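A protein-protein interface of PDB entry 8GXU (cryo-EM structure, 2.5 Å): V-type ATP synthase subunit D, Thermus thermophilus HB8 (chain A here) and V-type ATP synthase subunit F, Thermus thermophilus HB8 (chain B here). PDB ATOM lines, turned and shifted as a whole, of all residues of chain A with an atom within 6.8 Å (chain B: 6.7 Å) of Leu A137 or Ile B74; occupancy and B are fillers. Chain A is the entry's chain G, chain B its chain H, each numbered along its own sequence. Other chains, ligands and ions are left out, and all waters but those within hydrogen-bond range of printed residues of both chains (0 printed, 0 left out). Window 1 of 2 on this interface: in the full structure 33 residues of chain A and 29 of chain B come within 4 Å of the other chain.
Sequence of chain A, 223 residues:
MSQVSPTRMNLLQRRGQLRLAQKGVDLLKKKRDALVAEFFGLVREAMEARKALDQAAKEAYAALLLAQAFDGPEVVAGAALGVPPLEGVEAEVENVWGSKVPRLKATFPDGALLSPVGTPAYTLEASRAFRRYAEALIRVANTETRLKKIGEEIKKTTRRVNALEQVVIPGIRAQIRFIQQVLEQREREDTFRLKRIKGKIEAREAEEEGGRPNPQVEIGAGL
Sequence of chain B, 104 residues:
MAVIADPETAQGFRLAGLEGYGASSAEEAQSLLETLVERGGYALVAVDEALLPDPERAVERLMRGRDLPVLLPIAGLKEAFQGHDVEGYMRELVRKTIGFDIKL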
ATOM      1  N   ARG A  50       0.477 -33.791 -26.781  1.00  0.00           N
ATOM      2  CA  ARG A  50       1.881 -34.158 -26.655  1.00  0.00           C
ATOM      3  C   ARG A  50       2.624 -33.954 -27.965  1.00  0.00           C
ATOM      4  O   ARG A  50       3.786 -33.539 -27.962  1.00  0.00           O
ATOM      5  CB  ARG A  50       2.005 -35.606 -26.202  1.00  0.00           C
ATOM      6  CG  ARG A  50       2.083 -35.771 -24.707  1.00  0.00           C
ATOM      7  CD  ARG A  50       3.453 -35.438 -24.177  1.00  0.00           C
ATOM      8  NE  ARG A  50       3.463 -35.455 -22.721  1.00  0.00           N
ATOM      9  CZ  ARG A  50       4.487 -35.840 -21.976  1.00  0.00           C
ATOM     10  NH1 ARG A  50       5.635 -36.215 -22.515  1.00  0.00           N
ATOM     11  NH2 ARG A  50       4.359 -35.844 -20.653  1.00  0.00           N
ATOM     12  N   LEU A  53       3.309 -30.350 -28.201  1.00  0.00           N
ATOM     13  CA  LEU A  53       4.383 -29.984 -27.287  1.00  0.00           C
ATOM     14  C   LEU A  53       5.738 -30.393 -27.841  1.00  0.00           C
ATOM     15  O   LEU A  53       6.720 -29.665 -27.689  1.00  0.00           O
ATOM     16  CB  LEU A  53       4.154 -30.628 -25.922  1.00  0.00           C
ATOM     17  CG  LEU A  53       5.216 -30.334 -24.863  1.00  0.00           C
ATOM     18  CD1 LEU A  53       5.206 -28.856 -24.515  1.00  0.00           C
ATOM     19  CD2 LEU A  53       5.001 -31.181 -23.621  1.00  0.00           C
ATOM     20  N   ALA A  56       6.732 -27.929 -30.533  1.00  0.00           N
ATOM     21  CA  ALA A  56       7.148 -26.672 -29.929  1.00  0.00           C
ATOM     22  C   ALA A  56       8.513 -26.808 -29.273  1.00  0.00           C
ATOM     23  O   ALA A  56       9.333 -25.890 -29.334  1.00  0.00           O
ATOM     24  CB  ALA A  56       6.111 -26.205 -28.911  1.00  0.00           C
ATOM     25  N   ALA A  57       8.768 -27.940 -28.619  1.00  0.00           N
ATOM     26  CA  ALA A  57      10.073 -28.151 -28.008  1.00  0.00           C
ATOM     27  C   ALA A  57      11.163 -28.107 -29.063  1.00  0.00           C
ATOM     28  O   ALA A  57      12.206 -27.471 -28.868  1.00  0.00           O
ATOM     29  CB  ALA A  57      10.099 -29.487 -27.267  1.00  0.00           C
ATOM     30  N   LEU A 104      -4.674 -25.171 -14.814  1.00  0.00           N
ATOM     31  CA  LEU A 104      -3.775 -24.031 -14.830  1.00  0.00           C
ATOM     32  C   LEU A 104      -4.194 -23.049 -15.916  1.00  0.00           C
ATOM     33  O   LEU A 104      -4.410 -23.431 -17.070  1.00  0.00           O
ATOM     34  CB  LEU A 104      -2.343 -24.503 -15.054  1.00  0.00           C
ATOM     35  CG  LEU A 104      -1.864 -25.586 -14.086  1.00  0.00           C
ATOM     36  CD1 LEU A 104      -0.422 -25.966 -14.377  1.00  0.00           C
ATOM     37  CD2 LEU A 104      -2.019 -25.133 -12.645  1.00  0.00           C
ATOM     38  N   ARG A 132       5.838 -19.523 -25.822  1.00  0.00           N
ATOM     39  CA  ARG A 132       4.843 -20.373 -26.474  1.00  0.00           C
ATOM     40  C   ARG A 132       5.023 -21.836 -26.074  1.00  0.00           C
ATOM     41  O   ARG A 132       4.043 -22.579 -25.919  1.00  0.00           O
ATOM     42  CB  ARG A 132       4.925 -20.207 -27.988  1.00  0.00           C
ATOM     43  CG  ARG A 132       4.566 -18.806 -28.456  1.00  0.00           C
ATOM     44  CD  ARG A 132       4.269 -18.757 -29.946  1.00  0.00           C
ATOM     45  NE  ARG A 132       5.478 -18.840 -30.757  1.00  0.00           N
ATOM     46  CZ  ARG A 132       6.005 -19.967 -31.215  1.00  0.00           C
ATOM     47  NH1 ARG A 132       5.463 -21.145 -30.949  1.00  0.00           N
ATOM     48  NH2 ARG A 132       7.106 -19.912 -31.958  1.00  0.00           N
ATOM     49  N   TYR A 133       6.274 -22.265 -25.907  1.00  0.00           N
ATOM     50  CA  TYR A 133       6.544 -23.622 -25.456  1.00  0.00           C
ATOM     51  C   TYR A 133       5.961 -23.855 -24.071  1.00  0.00           C
ATOM     52  O   TYR A 133       5.397 -24.919 -23.793  1.00  0.00           O
ATOM     53  CB  TYR A 133       8.052 -23.862 -25.462  1.00  0.00           C
ATOM     54  CG  TYR A 133       8.477 -25.259 -25.099  1.00  0.00           C
ATOM     55  CD1 TYR A 133       7.764 -26.357 -25.539  1.00  0.00           C
ATOM     56  CD2 TYR A 133       9.596 -25.475 -24.314  1.00  0.00           C
ATOM     57  CE1 TYR A 133       8.154 -27.635 -25.207  1.00  0.00           C
ATOM     58  CE2 TYR A 133       9.994 -26.746 -23.977  1.00  0.00           C
ATOM     59  CZ  TYR A 133       9.271 -27.824 -24.427  1.00  0.00           C
ATOM     60  OH  TYR A 133       9.664 -29.100 -24.092  1.00  0.00           O
ATOM     61  N   ALA A 134       6.090 -22.865 -23.188  1.00  0.00           N
ATOM     62  CA  ALA A 134       5.491 -22.965 -21.863  1.00  0.00           C
ATOM     63  C   ALA A 134       3.974 -23.054 -21.956  1.00  0.00           C
ATOM     64  O   ALA A 134       3.337 -23.779 -21.183  1.00  0.00           O
ATOM     65  CB  ALA A 134       5.907 -21.769 -21.010  1.00  0.00           C
ATOM     66  N   GLU A 135       3.376 -22.313 -22.889  1.00  0.00           N
ATOM     67  CA  GLU A 135       1.932 -22.419 -23.093  1.00  0.00           C
ATOM     68  C   GLU A 135       1.535 -23.847 -23.464  1.00  0.00           C
ATOM     69  O   GLU A 135       0.602 -24.426 -22.884  1.00  0.00           O
ATOM     70  CB  GLU A 135       1.484 -21.442 -24.181  1.00  0.00           C
ATOM     71  CG  GLU A 135      -0.004 -21.139 -24.162  1.00  0.00           C
ATOM     72  CD  GLU A 135      -0.832 -22.200 -24.862  1.00  0.00           C
ATOM     73  OE1 GLU A 135      -0.350 -22.775 -25.861  1.00  0.00           O
ATOM     74  OE2 GLU A 135      -1.967 -22.464 -24.410  1.00  0.00           O
ATOM     75  N   ALA A 136       2.230 -24.428 -24.440  1.00  0.00           N
ATOM     76  CA  ALA A 136       1.902 -25.789 -24.850  1.00  0.00           C
ATOM     77  C   ALA A 136       2.125 -26.771 -23.707  1.00  0.00           C
ATOM     78  O   ALA A 136       1.363 -27.733 -23.541  1.00  0.00           O
ATOM     79  CB  ALA A 136       2.732 -26.185 -26.069  1.00  0.00           C
ATOM     80  N   LEU A 137       3.172 -26.548 -22.913  1.00  0.00           N
ATOM     81  CA  LEU A 137       3.433 -27.405 -21.764  1.00  0.00           C
ATOM     82  C   LEU A 137       2.291 -27.331 -20.759  1.00  0.00           C
ATOM     83  O   LEU A 137       1.885 -28.352 -20.184  1.00  0.00           O
ATOM     84  CB  LEU A 137       4.757 -26.998 -21.120  1.00  0.00           C
ATOM     85  CG  LEU A 137       5.320 -27.912 -20.037  1.00  0.00           C
ATOM     86  CD1 LEU A 137       5.704 -29.259 -20.621  1.00  0.00           C
ATOM     87  CD2 LEU A 137       6.515 -27.257 -19.366  1.00  0.00           C
ATOM     88  N   ILE A 138       1.748 -26.132 -20.544  1.00  0.00           N
ATOM     89  CA  ILE A 138       0.581 -25.986 -19.676  1.00  0.00           C
ATOM     90  C   ILE A 138      -0.594 -26.783 -20.224  1.00  0.00           C
ATOM     91  O   ILE A 138      -1.319 -27.448 -19.472  1.00  0.00           O
ATOM     92  CB  ILE A 138       0.224 -24.499 -19.513  1.00  0.00           C
ATOM     93  CG1 ILE A 138       0.966 -23.915 -18.313  1.00  0.00           C
ATOM     94  CG2 ILE A 138      -1.284 -24.319 -19.356  1.00  0.00           C
ATOM     95  CD1 ILE A 138       0.763 -22.425 -18.131  1.00  0.00           C
ATOM     96  N   ARG A 139      -0.823 -26.711 -21.533  1.00  0.00           N
ATOM     97  CA  ARG A 139      -1.932 -27.471 -22.105  1.00  0.00           C
ATOM     98  C   ARG A 139      -1.749 -28.968 -21.876  1.00  0.00           C
ATOM     99  O   ARG A 139      -2.705 -29.685 -21.532  1.00  0.00           O
ATOM    100  CB  ARG A 139      -2.065 -27.175 -23.594  1.00  0.00           C
ATOM    101  CG  ARG A 139      -3.450 -27.437 -24.135  1.00  0.00           C
ATOM    102  CD  ARG A 139      -3.578 -26.989 -25.583  1.00  0.00           C
ATOM    103  NE  ARG A 139      -3.324 -28.080 -26.518  1.00  0.00           N
ATOM    104  CZ  ARG A 139      -2.393 -28.072 -27.464  1.00  0.00           C
ATOM    105  NH1 ARG A 139      -1.577 -27.045 -27.633  1.00  0.00           N
ATOM    106  NH2 ARG A 139      -2.278 -29.127 -28.265  1.00  0.00           N
ATOM    107  N   VAL A 140      -0.525 -29.459 -22.067  1.00  0.00           N
ATOM    108  CA  VAL A 140      -0.254 -30.875 -21.849  1.00  0.00           C
ATOM    109  C   VAL A 140      -0.531 -31.250 -20.401  1.00  0.00           C
ATOM    110  O   VAL A 140      -1.110 -32.309 -20.118  1.00  0.00           O
ATOM    111  CB  VAL A 140       1.191 -31.207 -22.253  1.00  0.00           C
ATOM    112  CG1 VAL A 140       1.662 -32.475 -21.566  1.00  0.00           C
ATOM    113  CG2 VAL A 140       1.286 -31.347 -23.761  1.00  0.00           C
ATOM    114  N   ALA A 141      -0.120 -30.400 -19.462  1.00  0.00           N
ATOM    115  CA  ALA A 141      -0.406 -30.672 -18.058  1.00  0.00           C
ATOM    116  C   ALA A 141      -1.906 -30.752 -17.815  1.00  0.00           C
ATOM    117  O   ALA A 141      -2.387 -31.627 -17.077  1.00  0.00           O
ATOM    118  CB  ALA A 141       0.211 -29.587 -17.178  1.00  0.00           C
ATOM    119  N   ASN A 142      -2.657 -29.838 -18.424  1.00  0.00           N
ATOM    120  CA  ASN A 142      -4.098 -29.814 -18.220  1.00  0.00           C
ATOM    121  C   ASN A 142      -4.733 -31.108 -18.695  1.00  0.00           C
ATOM    122  O   ASN A 142      -5.627 -31.648 -18.037  1.00  0.00           O
ATOM    123  CB  ASN A 142      -4.710 -28.620 -18.945  1.00  0.00           C
ATOM    124  CG  ASN A 142      -4.713 -27.375 -18.099  1.00  0.00           C
ATOM    125  OD1 ASN A 142      -4.305 -27.400 -16.939  1.00  0.00           O
ATOM    126  ND2 ASN A 142      -5.174 -26.271 -18.672  1.00  0.00           N
ATOM    127  N   ALA B   2       7.878 -23.682 -12.349  1.00  0.00           N
ATOM    128  CA  ALA B   2       9.308 -23.946 -12.389  1.00  0.00           C
ATOM    129  C   ALA B   2       9.551 -25.125 -13.316  1.00  0.00           C
ATOM    130  O   ALA B   2       8.615 -25.787 -13.770  1.00  0.00           O
ATOM    131  CB  ALA B   2       9.868 -24.222 -10.990  1.00  0.00           C
ATOM    132  N   VAL B   3      10.827 -25.378 -13.597  1.00  0.00           N
ATOM    133  CA  VAL B   3      11.230 -26.506 -14.427  1.00  0.00           C
ATOM    134  C   VAL B   3      12.618 -26.953 -13.997  1.00  0.00           C
ATOM    135  O   VAL B   3      13.446 -26.149 -13.562  1.00  0.00           O
ATOM    136  CB  VAL B   3      11.213 -26.150 -15.933  1.00  0.00           C
ATOM    137  CG1 VAL B   3      11.765 -27.300 -16.758  1.00  0.00           C
ATOM    138  CG2 VAL B   3       9.807 -25.798 -16.386  1.00  0.00           C
ATOM    139  N   ILE B   4      12.867 -28.253 -14.122  1.00  0.00           N
ATOM    140  CA  ILE B   4      14.188 -28.839 -13.946  1.00  0.00           C
ATOM    141  C   ILE B   4      14.548 -29.569 -15.230  1.00  0.00           C
ATOM    142  O   ILE B   4      13.759 -30.380 -15.731  1.00  0.00           O
ATOM    143  CB  ILE B   4      14.236 -29.797 -12.743  1.00  0.00           C
ATOM    144  CG1 ILE B   4      13.943 -29.033 -11.448  1.00  0.00           C
ATOM    145  CG2 ILE B   4      15.585 -30.496 -12.678  1.00  0.00           C
ATOM    146  CD1 ILE B   4      13.650 -29.924 -10.257  1.00  0.00           C
ATOM    147  N   ALA B   5      15.729 -29.282 -15.762  1.00  0.00           N
ATOM    148  CA  ALA B   5      16.209 -29.932 -16.972  1.00  0.00           C
ATOM    149  C   ALA B   5      17.714 -29.703 -17.066  1.00  0.00           C
ATOM    150  O   ALA B   5      18.346 -29.216 -16.124  1.00  0.00           O
ATOM    151  CB  ALA B   5      15.463 -29.407 -18.203  1.00  0.00           C
ATOM    152  N   PHE B  13      14.378 -21.608 -20.589  1.00  0.00           N
ATOM    153  CA  PHE B  13      13.173 -21.606 -19.766  1.00  0.00           C
ATOM    154  C   PHE B  13      13.106 -20.348 -18.913  1.00  0.00           C
ATOM    155  O   PHE B  13      12.047 -19.720 -18.798  1.00  0.00           O
ATOM    156  CB  PHE B  13      13.134 -22.852 -18.880  1.00  0.00           C
ATOM    157  CG  PHE B  13      12.708 -24.102 -19.600  1.00  0.00           C
ATOM    158  CD1 PHE B  13      11.509 -24.146 -20.294  1.00  0.00           C
ATOM    159  CD2 PHE B  13      13.501 -25.236 -19.574  1.00  0.00           C
ATOM    160  CE1 PHE B  13      11.114 -25.294 -20.952  1.00  0.00           C
ATOM    161  CE2 PHE B  13      13.111 -26.388 -20.231  1.00  0.00           C
ATOM    162  CZ  PHE B  13      11.916 -26.417 -20.921  1.00  0.00           C
ATOM    163  N   LEU B  18      10.262 -18.819 -16.640  1.00  0.00           N
ATOM    164  CA  LEU B  18      10.112 -19.957 -15.745  1.00  0.00           C
ATOM    165  C   LEU B  18      11.356 -20.103 -14.880  1.00  0.00           C
ATOM    166  O   LEU B  18      12.478 -19.903 -15.347  1.00  0.00           O
ATOM    167  CB  LEU B  18       9.875 -21.243 -16.540  1.00  0.00           C
ATOM    168  CG  LEU B  18       8.671 -21.228 -17.485  1.00  0.00           C
ATOM    169  CD1 LEU B  18       8.590 -22.530 -18.266  1.00  0.00           C
ATOM    170  CD2 LEU B  18       7.383 -20.978 -16.718  1.00  0.00           C
ATOM    171  N   LEU B  44       3.583 -25.806 -10.885  1.00  0.00           N
ATOM    172  CA  LEU B  44       3.925 -26.735 -11.952  1.00  0.00           C
ATOM    173  C   LEU B  44       5.424 -26.979 -11.967  1.00  0.00           C
ATOM    174  O   LEU B  44       6.219 -26.041 -11.851  1.00  0.00           O
ATOM    175  CB  LEU B  44       3.482 -26.214 -13.314  1.00  0.00           C
ATOM    176  CG  LEU B  44       3.938 -27.068 -14.497  1.00  0.00           C
ATOM    177  CD1 LEU B  44       2.807 -27.237 -15.489  1.00  0.00           C
ATOM    178  CD2 LEU B  44       5.149 -26.452 -15.176  1.00  0.00           C
ATOM    179  N   VAL B  45       5.803 -28.246 -12.108  1.00  0.00           N
ATOM    180  CA  VAL B  45       7.205 -28.628 -12.191  1.00  0.00           C
ATOM    181  C   VAL B  45       7.369 -29.702 -13.256  1.00  0.00           C
ATOM    182  O   VAL B  45       7.097 -30.881 -13.009  1.00  0.00           O
ATOM    183  CB  VAL B  45       7.729 -29.128 -10.834  1.00  0.00           C
ATOM    184  CG1 VAL B  45       9.247 -29.164 -10.831  1.00  0.00           C
ATOM    185  CG2 VAL B  45       7.204 -28.261  -9.700  1.00  0.00           C
ATOM    186  N   ALA B  46       7.820 -29.310 -14.441  1.00  0.00           N
ATOM    187  CA  ALA B  46       8.135 -30.264 -15.493  1.00  0.00           C
ATOM    188  C   ALA B  46       9.559 -30.769 -15.321  1.00  0.00           C
ATOM    189  O   ALA B  46      10.487 -29.984 -15.109  1.00  0.00           O
ATOM    190  CB  ALA B  46       7.968 -29.626 -16.871  1.00  0.00           C
ATOM    191  N   VAL B  47       9.728 -32.084 -15.414  1.00  0.00           N
ATOM    192  CA  VAL B  47      11.002 -32.745 -15.150  1.00  0.00           C
ATOM    193  C   VAL B  47      11.475 -33.414 -16.429  1.00  0.00           C
ATOM    194  O   VAL B  47      10.702 -34.115 -17.092  1.00  0.00           O
ATOM    195  CB  VAL B  47      10.879 -33.778 -14.017  1.00  0.00           C
ATOM    196  CG1 VAL B  47      12.191 -34.520 -13.828  1.00  0.00           C
ATOM    197  CG2 VAL B  47      10.449 -33.099 -12.724  1.00  0.00           C
ATOM    198  N   ASP B  48      12.739 -33.193 -16.779  1.00  0.00           N
ATOM    199  CA  ASP B  48      13.297 -33.829 -17.963  1.00  0.00           C
ATOM    200  C   ASP B  48      13.208 -35.342 -17.825  1.00  0.00           C
ATOM    201  O   ASP B  48      13.615 -35.912 -16.809  1.00  0.00           O
ATOM    202  CB  ASP B  48      14.747 -33.393 -18.169  1.00  0.00           C
ATOM    203  CG  ASP B  48      15.592 -33.569 -16.923  1.00  0.00           C
ATOM    204  OD1 ASP B  48      15.019 -33.587 -15.813  1.00  0.00           O
ATOM    205  OD2 ASP B  48      16.828 -33.682 -17.056  1.00  0.00           O
ATOM    206  N   GLU B  49      12.667 -35.990 -18.858  1.00  0.00           N
ATOM    207  CA  GLU B  49      12.438 -37.429 -18.788  1.00  0.00           C
ATOM    208  C   GLU B  49      13.749 -38.191 -18.659  1.00  0.00           C
ATOM    209  O   GLU B  49      13.850 -39.137 -17.870  1.00  0.00           O
ATOM    210  CB  GLU B  49      11.674 -37.892 -20.029  1.00  0.00           C
ATOM    211  CG  GLU B  49      11.061 -39.277 -19.901  1.00  0.00           C
ATOM    212  CD  GLU B  49      10.352 -39.717 -21.166  1.00  0.00           C
ATOM    213  OE1 GLU B  49       9.870 -38.842 -21.916  1.00  0.00           O
ATOM    214  OE2 GLU B  49      10.278 -40.940 -21.414  1.00  0.00           O
ATOM    215  N   ALA B  50      14.767 -37.784 -19.419  1.00  0.00           N
ATOM    216  CA  ALA B  50      16.001 -38.558 -19.489  1.00  0.00           C
ATOM    217  C   ALA B  50      16.605 -38.768 -18.109  1.00  0.00           C
ATOM    218  O   ALA B  50      17.105 -39.856 -17.800  1.00  0.00           O
ATOM    219  CB  ALA B  50      17.001 -37.861 -20.411  1.00  0.00           C
ATOM    220  N   PRO B  55       8.656 -38.774 -12.662  1.00  0.00           N
ATOM    221  CA  PRO B  55       8.786 -37.919 -11.470  1.00  0.00           C
ATOM    222  C   PRO B  55       7.764 -38.236 -10.397  1.00  0.00           C
ATOM    223  O   PRO B  55       8.086 -38.181  -9.205  1.00  0.00           O
ATOM    224  CB  PRO B  55       8.608 -36.499 -12.026  1.00  0.00           C
ATOM    225  CG  PRO B  55       8.003 -36.645 -13.361  1.00  0.00           C
ATOM    226  CD  PRO B  55       8.228 -38.033 -13.856  1.00  0.00           C
ATOM    227  N   LEU B  72       5.398 -33.355 -14.410  1.00  0.00           N
ATOM    228  CA  LEU B  72       5.203 -33.554 -15.836  1.00  0.00           C
ATOM    229  C   LEU B  72       6.488 -34.065 -16.472  1.00  0.00           C
ATOM    230  O   LEU B  72       7.540 -33.432 -16.324  1.00  0.00           O
ATOM    231  CB  LEU B  72       4.765 -32.245 -16.486  1.00  0.00           C
ATOM    232  CG  LEU B  72       4.035 -32.347 -17.821  1.00  0.00           C
ATOM    233  CD1 LEU B  72       3.298 -31.058 -18.101  1.00  0.00           C
ATOM    234  CD2 LEU B  72       5.001 -32.664 -18.944  1.00  0.00           C
ATOM    235  N   PRO B  73       6.462 -35.204 -17.165  1.00  0.00           N
ATOM    236  CA  PRO B  73       7.642 -35.616 -17.940  1.00  0.00           C
ATOM    237  C   PRO B  73       7.741 -34.819 -19.232  1.00  0.00           C
ATOM    238  O   PRO B  73       6.855 -34.885 -20.087  1.00  0.00           O
ATOM    239  CB  PRO B  73       7.394 -37.105 -18.209  1.00  0.00           C
ATOM    240  CG  PRO B  73       6.313 -37.509 -17.265  1.00  0.00           C
ATOM    241  CD  PRO B  73       5.479 -36.292 -17.059  1.00  0.00           C
ATOM    242  N   ILE B  74       8.829 -34.072 -19.375  1.00  0.00           N
ATOM    243  CA  ILE B  74       9.066 -33.237 -20.543  1.00  0.00           C
ATOM    244  C   ILE B  74      10.196 -33.847 -21.357  1.00  0.00           C
ATOM    245  O   ILE B  74      11.105 -34.484 -20.816  1.00  0.00           O
ATOM    246  CB  ILE B  74       9.387 -31.784 -20.136  1.00  0.00           C
ATOM    247  CG1 ILE B  74       9.250 -30.851 -21.339  1.00  0.00           C
ATOM    248  CG2 ILE B  74      10.776 -31.695 -19.535  1.00  0.00           C
ATOM    249  CD1 ILE B  74       9.268 -29.382 -20.973  1.00  0.00           C
ATOM    250  N   ALA B  75      10.131 -33.650 -22.669  1.00  0.00           N
ATOM    251  CA  ALA B  75      11.059 -34.309 -23.577  1.00  0.00           C
ATOM    252  C   ALA B  75      12.462 -33.722 -23.460  1.00  0.00           C
ATOM    253  O   ALA B  75      12.645 -32.537 -23.172  1.00  0.00           O
ATOM    254  CB  ALA B  75      10.567 -34.191 -25.018  1.00  0.00           C
ATOM    255  N   GLY B  76      13.459 -34.572 -23.696  1.00  0.00           N
ATOM    256  CA  GLY B  76      14.839 -34.134 -23.681  1.00  0.00           C
ATOM    257  C   GLY B  76      15.206 -33.352 -24.929  1.00  0.00           C
ATOM    258  O   GLY B  76      14.490 -33.330 -25.931  1.00  0.00           O
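Of chain B, only Ala B46, Leu B72 and Ile B74 come within 4 Å of Leu A137.
Printed residues of chain B within 4 Å of Ala A141: Leu B44 and Leu B72.
Of the printed residues of chain A, Leu B18 touches Ala A134 (3.9 Å).
Of the printed residues of chain A, Ala B46 touches Leu A137 (3.7 Å).
Of the printed residues of chain A, Ile B74 touches Tyr A133 (3.2 Å) and Leu A137 (3.6 Å).
The nearest printed residue of chain A that does not touch Pro B73 is Leu A53 (5.4 Å).
Leu B72 touches Arg A50.
CD1 of Leu A104 touches CD1 of Leu B44, 3.6 Å away.
CE1 of Phe B13 touches CE2 of Tyr A133, 3.5 Å away.
Ile B74 touches Tyr A133 (CD1 to OH, 3.2 Å).
CD1 of Leu B18 touches CB of Ala A134, at 3.9 Å.
CD2 of Leu A137 touches CB of Ala B46, 3.7 Å away.
CD1 of Leu B72 touches O of Leu A137, at 3.7 Å.
CD1 of Ile B74 touches CD1 of Leu A137, at 3.6 Å.
CB of Ala A141 touches CD1 of Leu B44 (3.9 Å).
Ala A141 touches Leu B72.
N of Ala B2 lies within hydrogen-bond range of O of Leu B44 (2.9 Å).
The backbone NH (N) of Ile B4 sits at hydrogen-bond distance from the backbone carbonyl oxygen (O) of Ala B46 (3.1 Å).
O of Phe B13 lies within hydrogen-bond range of N of Leu B18.
N of Val B47 is in hydrogen-bond range of O of Leu B72 (2.7 Å).
The backbone carbonyl oxygen (O) of Val B47 is in hydrogen-bond range of the backbone NH (N) of Ile B74, at 3.0 Å.
The backbone carbonyl oxygen (O) of Ile B74 lies within hydrogen-bond range of the backbone NH (N) of Glu B49 (2.9 Å).
The guanidinium group (NH2) of Arg A50 lies within hydrogen-bond range of the backbone carbonyl oxygen (O) of Pro B73 (2.7 Å).
Of the 16 printed residues of chain A, 6 touch a printed residue of chain B.
Printed residues of chain B that touch a printed residue of chain A: Phe B13, Leu B18, Leu B44, Ala B46, Leu B72, Pro B73 and Ile B74.
Hydrophobic or aromatic side chains of chain B within 4 Å of the printed part of chain A: Phe B13, Leu B18, Leu B44, Ala B46, Leu B72, Pro B73 and Ile B74.
Among the printed residues, 11 pairs touch across the chains.
Among the printed residues, no Asp or Glu carboxylate lies within 4 Å of a Lys or Arg side-chain nitrogen of the other chain.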
